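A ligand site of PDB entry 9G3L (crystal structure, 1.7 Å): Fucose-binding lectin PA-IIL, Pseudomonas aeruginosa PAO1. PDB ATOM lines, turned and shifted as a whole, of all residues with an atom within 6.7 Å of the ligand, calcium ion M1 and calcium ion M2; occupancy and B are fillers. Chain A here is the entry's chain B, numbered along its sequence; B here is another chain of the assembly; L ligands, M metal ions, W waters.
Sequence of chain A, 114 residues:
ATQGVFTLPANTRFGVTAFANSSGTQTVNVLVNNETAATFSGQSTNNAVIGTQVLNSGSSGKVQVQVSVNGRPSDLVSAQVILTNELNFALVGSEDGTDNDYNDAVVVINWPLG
Of the 26 residues printed, 5 come within 4 Å of calcium ion M2.
Along chain A the residues within 4 Å of calcium ion M2 span positions 21 to 104.
Calcium ion M1 is bound by the side-chain carboxylate (OD1) of Asp 99 (2.3 Å), the side-chain carboxylate (OD1) of Asp 101 (2.4 Å), the side-chain carboxylate (OE2) of Glu 95 (2.4 Å), the side-chain carboxylate (OD2) of Asp 104 (2.4 Å), an oxygen (O4) of the ligand (2.4 Å), the side-chain carboxylate (OE1) of Glu 95 (2.5 Å), an oxygen (O5) of the ligand (2.6 Å) and the side-chain carboxylate (OD1) of Asp 104 (2.6 Å).
Calcium ion M1 has eight donor atoms within binding distance.
Water W2 lies within hydrogen-bond range of an oxygen (O1) of the ligand and the side-chain hydroxyl (OG) of Ser 23.
Within 4 Å of calcium ion M1: Glu 95, Asp 99, Asp 101 and Asp 104.
The nearest printed residue that does not touch calcium ion M1 is Asp 96 (4.1 Å).
N2 of the ligand sits at hydrogen-bond distance from OD1 of Asp 96, 3.2 Å away.
A nitrogen (N2) of the ligand is in hydrogen-bond range of the side-chain hydroxyl (OG) of Ser 22 (3.0 Å).
The backbone NH of Ser 23 lies within hydrogen-bond range of an oxygen (O2) of the ligand.
Residues that only touch the ligand: Gly 24, Thr 45, Val 69, Asn 70 and Gly 97.
Hydrophobic or aromatic side chains that line the ligand: Val 69.
Along chain A the residues within 4 Å of the ligand span positions 21 to 104.
O of Asn 21 binds calcium ion M2 (2.3 Å).
OD1 of Asn 103 binds calcium ion M2 (2.3 Å).
OD1 of Asp 104 is bound to calcium ion M2, 2.4 Å away.
Calcium ion M2 is bound by O of Gly 114 of chain B.
OD2 of Asp 101 binds calcium ion M2 (2.5 Å).
O4 of the ligand binds calcium ion M2, 2.5 Å away.
Calcium ion M2 is bound by O3 of the ligand (2.5 Å).
Calcium ion M2 has seven donor atoms within binding distance.
Slightly farther from calcium ion M2 lies the side-chain carboxylate (OD1) of Asp 101 (3.0 Å).
The backbone carbonyl oxygen (O) of Ser 44 sits close to the backbone NH (N) of Asn 21.
ND2 of Asn 103 sits close to O of Leu 113 of chain B (3.3 Å).
O of Pro 112 of chain B is in hydrogen-bond range of ND2 of Asn 103 (2.8 Å).
N of Asp 96 sits close to OD2 of Asp 104 (2.8 Å).
OE2 of Glu 95 sits close to N of Gly 97, at 2.8 Å.
OE1 of Glu 95 sits close to N of Tyr 102, 3.0 Å away.
The backbone NH of Asn 100 sits close to the side-chain carboxylate of Glu 95.
The side-chain amide nitrogen of Gln 26 sits at hydrogen-bond distance from the side-chain carboxylate of Asp 96.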
ATOM      1  N   ASN A  21       1.787  15.729  -6.409  1.00  0.00           N
ATOM      2  CA  ASN A  21       2.201  14.921  -5.264  1.00  0.00           C
ATOM      3  C   ASN A  21       1.249  15.160  -4.100  1.00  0.00           C
ATOM      4  O   ASN A  21       1.618  15.749  -3.073  1.00  0.00           O
ATOM      5  CB  ASN A  21       3.646  15.221  -4.817  1.00  0.00           C
ATOM      6  CG  ASN A  21       4.681  14.715  -5.804  1.00  0.00           C
ATOM      7  OD1 ASN A  21       4.949  13.499  -5.901  1.00  0.00           O
ATOM      8  ND2 ASN A  21       5.203  15.622  -6.615  1.00  0.00           N
ATOM      9  N   SER A  22      -0.011  14.755  -4.264  1.00  0.00           N
ATOM     10  CA  SER A  22      -1.026  15.031  -3.230  1.00  0.00           C
ATOM     11  C   SER A  22      -2.243  14.136  -3.415  1.00  0.00           C
ATOM     12  O   SER A  22      -2.453  13.673  -4.542  1.00  0.00           O
ATOM     13  CB  SER A  22      -1.504  16.492  -3.310  1.00  0.00           C
ATOM     14  OG  SER A  22      -2.556  16.770  -2.417  1.00  0.00           O
ATOM     15  N   SER A  23      -3.059  13.981  -2.352  1.00  0.00           N
ATOM     16  CA  SER A  23      -4.359  13.336  -2.501  1.00  0.00           C
ATOM     17  C   SER A  23      -5.345  14.276  -3.192  1.00  0.00           C
ATOM     18  O   SER A  23      -6.399  13.805  -3.677  1.00  0.00           O
ATOM     19  CB  SER A  23      -4.909  12.904  -1.159  1.00  0.00           C
ATOM     20  OG  SER A  23      -4.158  11.756  -0.733  1.00  0.00           O
ATOM     21  N   GLY A  24      -5.059  15.578  -3.155  1.00  0.00           N
ATOM     22  CA  GLY A  24      -5.906  16.569  -3.820  1.00  0.00           C
ATOM     23  C   GLY A  24      -5.625  16.740  -5.323  1.00  0.00           C
ATOM     24  O   GLY A  24      -4.465  16.682  -5.733  1.00  0.00           O
ATOM     25  N   THR A  25      -6.687  16.925  -6.106  1.00  0.00           N
ATOM     26  CA  THR A  25      -6.572  17.243  -7.528  1.00  0.00           C
ATOM     27  C   THR A  25      -5.981  18.626  -7.690  1.00  0.00           C
ATOM     28  O   THR A  25      -6.542  19.615  -7.223  1.00  0.00           O
ATOM     29  CB  THR A  25      -7.908  17.103  -8.275  1.00  0.00           C
ATOM     30  OG1 THR A  25      -8.389  15.756  -8.142  1.00  0.00           O
ATOM     31  CG2 THR A  25      -7.772  17.559  -9.734  1.00  0.00           C
ATOM     32  N   GLN A  26      -4.839  18.706  -8.382  1.00  0.00           N
ATOM     33  CA  GLN A  26      -4.218  20.025  -8.626  1.00  0.00           C
ATOM     34  C   GLN A  26      -4.749  20.676  -9.882  1.00  0.00           C
ATOM     35  O   GLN A  26      -4.912  19.987 -10.910  1.00  0.00           O
ATOM     36  CB  GLN A  26      -2.716  19.794  -8.795  1.00  0.00           C
ATOM     37  CG  GLN A  26      -2.086  19.047  -7.622  1.00  0.00           C
ATOM     38  CD  GLN A  26      -2.240  19.782  -6.318  1.00  0.00           C
ATOM     39  OE1 GLN A  26      -1.841  20.940  -6.212  1.00  0.00           O
ATOM     40  NE2 GLN A  26      -2.754  19.115  -5.308  1.00  0.00           N
ATOM     41  N   SER A  44      -2.101  12.860  -8.311  1.00  0.00           N
ATOM     42  CA  SER A  44      -1.062  11.849  -8.224  1.00  0.00           C
ATOM     43  C   SER A  44      -0.364  12.018  -6.884  1.00  0.00           C
ATOM     44  O   SER A  44      -0.121  13.153  -6.488  1.00  0.00           O
ATOM     45  CB  SER A  44      -0.017  11.964  -9.355  1.00  0.00           C
ATOM     46  OG  SER A  44       0.952  10.941  -9.277  1.00  0.00           O
ATOM     47  N   THR A  45       0.073  10.907  -6.298  1.00  0.00           N
ATOM     48  CA  THR A  45       1.009  10.934  -5.183  1.00  0.00           C
ATOM     49  C   THR A  45       2.319  10.305  -5.636  1.00  0.00           C
ATOM     50  O   THR A  45       3.158   9.962  -4.799  1.00  0.00           O
ATOM     51  CB  THR A  45       0.506  10.186  -3.931  1.00  0.00           C
ATOM     52  OG1 THR A  45       0.065   8.908  -4.381  1.00  0.00           O
ATOM     53  CG2 THR A  45      -0.590  10.951  -3.243  1.00  0.00           C
ATOM     54  N   VAL A  69      -6.624  23.914  -5.496  1.00  0.00           N
ATOM     55  CA  VAL A  69      -7.195  22.593  -5.338  1.00  0.00           C
ATOM     56  C   VAL A  69      -8.690  22.779  -5.045  1.00  0.00           C
ATOM     57  O   VAL A  69      -9.038  23.405  -4.059  1.00  0.00           O
ATOM     58  CB  VAL A  69      -6.451  21.797  -4.237  1.00  0.00           C
ATOM     59  CG1 VAL A  69      -7.103  20.437  -4.009  1.00  0.00           C
ATOM     60  CG2 VAL A  69      -4.969  21.641  -4.573  1.00  0.00           C
ATOM     61  N   ASN A  70      -9.568  22.292  -5.957  1.00  0.00           N
ATOM     62  CA  ASN A  70     -11.010  22.385  -5.725  1.00  0.00           C
ATOM     63  C   ASN A  70     -11.396  23.841  -5.432  1.00  0.00           C
ATOM     64  O   ASN A  70     -12.151  24.101  -4.481  1.00  0.00           O
ATOM     65  CB  ASN A  70     -11.476  21.394  -4.677  1.00  0.00           C
ATOM     66  CG  ASN A  70     -11.379  19.974  -5.142  1.00  0.00           C
ATOM     67  OD1 ASN A  70     -11.276  19.716  -6.345  1.00  0.00           O
ATOM     68  ND2 ASN A  70     -11.400  19.072  -4.202  1.00  0.00           N
ATOM     69  N   ARG A  72      -9.578  26.207  -4.163  1.00  0.00           N
ATOM     70  CA  ARG A  72      -8.807  26.878  -3.095  1.00  0.00           C
ATOM     71  C   ARG A  72      -7.331  27.086  -3.539  1.00  0.00           C
ATOM     72  O   ARG A  72      -6.646  26.126  -3.751  1.00  0.00           O
ATOM     73  CB  ARG A  72      -8.765  26.078  -1.813  1.00  0.00           C
ATOM     74  CG  ARG A  72     -10.095  26.106  -1.097  1.00  0.00           C
ATOM     75  CD  ARG A  72     -10.033  25.336   0.189  1.00  0.00           C
ATOM     76  NE  ARG A  72     -10.707  26.106   1.241  1.00  0.00           N
ATOM     77  CZ  ARG A  72     -10.151  27.008   2.009  1.00  0.00           C
ATOM     78  NH1 ARG A  72     -10.924  27.768   2.767  1.00  0.00           N
ATOM     79  NH2 ARG A  72      -8.844  27.155   2.019  1.00  0.00           N
ATOM     80  N   SER A  94       4.107  24.314  -4.072  1.00  0.00           N
ATOM     81  CA  SER A  94       2.758  24.674  -3.612  1.00  0.00           C
ATOM     82  C   SER A  94       2.329  23.748  -2.493  1.00  0.00           C
ATOM     83  O   SER A  94       2.643  22.566  -2.533  1.00  0.00           O
ATOM     84  CB  SER A  94       1.735  24.670  -4.751  1.00  0.00           C
ATOM     85  OG  SER A  94       1.532  23.401  -5.270  1.00  0.00           O
ATOM     86  N   GLU A  95       1.568  24.276  -1.509  1.00  0.00           N
ATOM     87  CA  GLU A  95       1.089  23.493  -0.388  1.00  0.00           C
ATOM     88  C   GLU A  95      -0.445  23.625  -0.310  1.00  0.00           C
ATOM     89  O   GLU A  95      -0.946  24.759  -0.227  1.00  0.00           O
ATOM     90  CB  GLU A  95       1.719  23.921   0.937  1.00  0.00           C
ATOM     91  CG  GLU A  95       1.170  23.229   2.182  1.00  0.00           C
ATOM     92  CD  GLU A  95       1.382  21.730   2.054  1.00  0.00           C
ATOM     93  OE1 GLU A  95       2.504  21.314   1.740  1.00  0.00           O
ATOM     94  OE2 GLU A  95       0.383  21.004   2.258  1.00  0.00           O
ATOM     95  N   ASP A  96      -1.160  22.494  -0.311  1.00  0.00           N
ATOM     96  CA  ASP A  96      -2.613  22.489  -0.298  1.00  0.00           C
ATOM     97  C   ASP A  96      -3.167  22.022   1.046  1.00  0.00           C
ATOM     98  O   ASP A  96      -4.393  21.807   1.147  1.00  0.00           O
ATOM     99  CB  ASP A  96      -3.122  21.617  -1.439  1.00  0.00           C
ATOM    100  CG  ASP A  96      -2.764  20.146  -1.404  1.00  0.00           C
ATOM    101  OD1 ASP A  96      -2.360  19.631  -0.322  1.00  0.00           O
ATOM    102  OD2 ASP A  96      -2.888  19.478  -2.451  1.00  0.00           O
ATOM    103  N   GLY A  97      -2.300  21.762   1.991  1.00  0.00           N
ATOM    104  CA  GLY A  97      -2.657  21.047   3.233  1.00  0.00           C
ATOM    105  C   GLY A  97      -1.876  21.582   4.450  1.00  0.00           C
ATOM    106  O   GLY A  97      -1.574  22.773   4.534  1.00  0.00           O
ATOM    107  N   THR A  98      -1.554  20.674   5.367  1.00  0.00           N
ATOM    108  CA  THR A  98      -0.974  21.033   6.637  1.00  0.00           C
ATOM    109  C   THR A  98       0.435  20.500   6.823  1.00  0.00           C
ATOM    110  O   THR A  98       1.074  20.883   7.806  1.00  0.00           O
ATOM    111  CB  THR A  98      -1.917  20.521   7.758  1.00  0.00           C
ATOM    112  OG1 THR A  98      -1.963  19.100   7.616  1.00  0.00           O
ATOM    113  CG2 THR A  98      -3.239  21.261   7.701  1.00  0.00           C
ATOM    114  N   ASP A  99       0.925  19.624   5.936  1.00  0.00           N
ATOM    115  CA  ASP A  99       2.215  18.961   6.175  1.00  0.00           C
ATOM    116  C   ASP A  99       3.427  19.784   5.760  1.00  0.00           C
ATOM    117  O   ASP A  99       4.544  19.433   6.120  1.00  0.00           O
ATOM    118  CB  ASP A  99       2.273  17.574   5.562  1.00  0.00           C
ATOM    119  CG  ASP A  99       2.250  17.525   4.047  1.00  0.00           C
ATOM    120  OD1 ASP A  99       1.912  18.557   3.444  1.00  0.00           O
ATOM    121  OD2 ASP A  99       2.563  16.435   3.500  1.00  0.00           O
ATOM    122  N   ASN A 100       3.215  20.804   4.920  1.00  0.00           N
ATOM    123  CA  ASN A 100       4.260  21.719   4.493  1.00  0.00           C
ATOM    124  C   ASN A 100       5.354  21.000   3.724  1.00  0.00           C
ATOM    125  O   ASN A 100       6.538  21.366   3.876  1.00  0.00           O
ATOM    126  CB  ASN A 100       4.804  22.546   5.642  1.00  0.00           C
ATOM    127  CG  ASN A 100       3.720  23.414   6.219  1.00  0.00           C
ATOM    128  OD1 ASN A 100       2.832  23.851   5.501  1.00  0.00           O
ATOM    129  ND2 ASN A 100       3.715  23.594   7.526  1.00  0.00           N
ATOM    130  N   ASP A 101       4.977  20.060   2.851  1.00  0.00           N
ATOM    131  CA  ASP A 101       5.978  19.480   1.954  1.00  0.00           C
ATOM    132  C   ASP A 101       6.149  20.380   0.705  1.00  0.00           C
ATOM    133  O   ASP A 101       7.177  20.245   0.023  1.00  0.00           O
ATOM    134  CB  ASP A 101       5.769  18.010   1.681  1.00  0.00           C
ATOM    135  CG  ASP A 101       4.483  17.622   0.955  1.00  0.00           C
ATOM    136  OD1 ASP A 101       3.680  18.497   0.656  1.00  0.00           O
ATOM    137  OD2 ASP A 101       4.336  16.395   0.662  1.00  0.00           O
ATOM    138  N   TYR A 102       5.183  21.226   0.428  1.00  0.00           N
ATOM    139  CA  TYR A 102       5.252  22.173  -0.697  1.00  0.00           C
ATOM    140  C   TYR A 102       5.517  21.520  -2.054  1.00  0.00           C
ATOM    141  O   TYR A 102       5.894  22.211  -2.984  1.00  0.00           O
ATOM    142  CB  TYR A 102       6.283  23.291  -0.337  1.00  0.00           C
ATOM    143  CG  TYR A 102       5.608  24.356   0.490  1.00  0.00           C
ATOM    144  CD1 TYR A 102       5.478  24.221   1.883  1.00  0.00           C
ATOM    145  CD2 TYR A 102       4.961  25.431  -0.104  1.00  0.00           C
ATOM    146  CE1 TYR A 102       4.790  25.166   2.634  1.00  0.00           C
ATOM    147  CE2 TYR A 102       4.267  26.349   0.643  1.00  0.00           C
ATOM    148  CZ  TYR A 102       4.170  26.230   2.010  1.00  0.00           C
ATOM    149  OH  TYR A 102       3.500  27.163   2.771  1.00  0.00           O
ATOM    150  N   ASN A 103       5.119  20.242  -2.201  1.00  0.00           N
ATOM    151  CA  ASN A 103       5.314  19.505  -3.446  1.00  0.00           C
ATOM    152  C   ASN A 103       3.979  19.141  -4.089  1.00  0.00           C
ATOM    153  O   ASN A 103       3.975  18.377  -5.051  1.00  0.00           O
ATOM    154  CB  ASN A 103       6.138  18.245  -3.222  1.00  0.00           C
ATOM    155  CG  ASN A 103       5.378  17.145  -2.529  1.00  0.00           C
ATOM    156  OD1 ASN A 103       4.249  17.390  -2.099  1.00  0.00           O
ATOM    157  ND2 ASN A 103       5.988  15.992  -2.350  1.00  0.00           N
ATOM    158  N   ASP A 104       2.854  19.678  -3.531  1.00  0.00           N
ATOM    159  CA  ASP A 104       1.548  19.171  -3.927  1.00  0.00           C
ATOM    160  C   ASP A 104       1.342  19.392  -5.429  1.00  0.00           C
ATOM    161  O   ASP A 104       0.826  18.487  -6.122  1.00  0.00           O
ATOM    162  CB  ASP A 104       0.502  19.774  -3.011  1.00  0.00           C
ATOM    163  CG  ASP A 104       0.742  19.447  -1.542  1.00  0.00           C
ATOM    164  OD1 ASP A 104       1.246  18.287  -1.267  1.00  0.00           O
ATOM    165  OD2 ASP A 104       0.597  20.310  -0.689  1.00  0.00           O
ATOM    166  N   ALA A 105       1.683  20.597  -5.900  1.00  0.00           N
ATOM    167  CA  ALA A 105       1.922  20.799  -7.331  1.00  0.00           C
ATOM    168  C   ALA A 105       3.299  21.472  -7.410  1.00  0.00           C
ATOM    169  O   ALA A 105       3.547  22.399  -6.664  1.00  0.00           O
ATOM    170  CB  ALA A 105       0.890  21.669  -8.019  1.00  0.00           C
ATOM    171  N   PRO B 112      10.959  16.291  -1.979  1.00  0.00           N
ATOM    172  CA  PRO B 112      10.289  15.014  -1.866  1.00  0.00           C
ATOM    173  C   PRO B 112       9.117  14.828  -2.823  1.00  0.00           C
ATOM    174  O   PRO B 112       8.556  15.785  -3.393  1.00  0.00           O
ATOM    175  CB  PRO B 112       9.722  15.144  -0.414  1.00  0.00           C
ATOM    176  CG  PRO B 112       9.397  16.574  -0.273  1.00  0.00           C
ATOM    177  CD  PRO B 112      10.640  17.196  -0.859  1.00  0.00           C
ATOM    178  N   LEU B 113       8.736  13.568  -2.969  1.00  0.00           N
ATOM    179  CA  LEU B 113       7.507  13.206  -3.655  1.00  0.00           C
ATOM    180  C   LEU B 113       6.388  12.890  -2.669  1.00  0.00           C
ATOM    181  O   LEU B 113       6.626  12.839  -1.455  1.00  0.00           O
ATOM    182  CB  LEU B 113       7.800  11.964  -4.509  1.00  0.00           C
ATOM    183  CG  LEU B 113       8.935  12.082  -5.534  1.00  0.00           C
ATOM    184  CD1 LEU B 113       8.895  10.939  -6.495  1.00  0.00           C
ATOM    185  CD2 LEU B 113       8.721  13.443  -6.280  1.00  0.00           C
ATOM    186  N   GLY B 114       5.189  12.620  -3.194  1.00  0.00           N
ATOM    187  CA  GLY B 114       4.112  12.090  -2.345  1.00  0.00           C
ATOM    188  C   GLY B 114       3.263  13.116  -1.648  1.00  0.00           C
ATOM    189  O   GLY B 114       3.660  14.305  -1.550  1.00  0.00           O
ATOM    190  OXT GLY B 114       2.137  12.707  -1.257  1.00  0.00           O
HETATM  191  O1  LIG L   1      -4.779  15.408   1.670  1.00  0.00           O
HETATM  192  C1  LIG L   1      -4.600  16.272   0.858  1.00  0.00           C
HETATM  193  C2  LIG L   1      -5.697  17.041   0.309  1.00  0.00           C
HETATM  194  C3  LIG L   1      -5.541  18.400  -0.022  1.00  0.00           C
HETATM  195  C4  LIG L   1      -6.579  19.139  -0.567  1.00  0.00           C
HETATM  196  C5  LIG L   1      -7.758  18.476  -0.820  1.00  0.00           C
HETATM  197  N1  LIG L   1      -8.934  18.932  -1.356  1.00  0.00           N
HETATM  198  C6  LIG L   1      -9.842  17.875  -1.469  1.00  0.00           C
HETATM  199  C7  LIG L   1      -9.399  16.772  -0.912  1.00  0.00           C
HETATM  200  C8  LIG L   1      -7.905  17.119  -0.528  1.00  0.00           C
HETATM  201  C9  LIG L   1      -6.901  16.416   0.031  1.00  0.00           C
HETATM  202  N2  LIG L   1      -3.294  16.628   0.437  1.00  0.00           N
HETATM  203  C10 LIG L   1      -2.201  15.947   0.995  1.00  0.00           C
HETATM  204  O2  LIG L   1      -2.067  14.685   0.339  1.00  0.00           O
HETATM  205  C11 LIG L   1      -1.092  13.840   0.993  1.00  0.00           C
HETATM  206  C12 LIG L   1      -1.143  12.560   0.308  1.00  0.00           C
HETATM  207  C13 LIG L   1       0.275  14.572   0.938  1.00  0.00           C
HETATM  208  O3  LIG L   1       0.768  14.594  -0.407  1.00  0.00           O
HETATM  209  C14 LIG L   1       0.158  15.975   1.464  1.00  0.00           C
HETATM  210  O4  LIG L   1       1.467  16.628   1.259  1.00  0.00           O
HETATM  211  C15 LIG L   1      -0.908  16.737   0.770  1.00  0.00           C
HETATM  212  O5  LIG L   1      -0.969  18.078   1.285  1.00  0.00           O
HETATM  213 CA    CA M   1       1.434  19.073   1.234  1.00  0.00          CA
HETATM  214 CA    CA M   2       2.494  16.305  -0.980  1.00  0.00          CA
HETATM  215  O   HOH W   1      -5.380  17.724   4.004  1.00  0.00           O
HETATM  216  O   HOH W   2      -4.097  12.899   2.464  1.00  0.00           O
HETATM  217  O   HOH W   3      -1.170  17.984   4.185  1.00  0.00           O
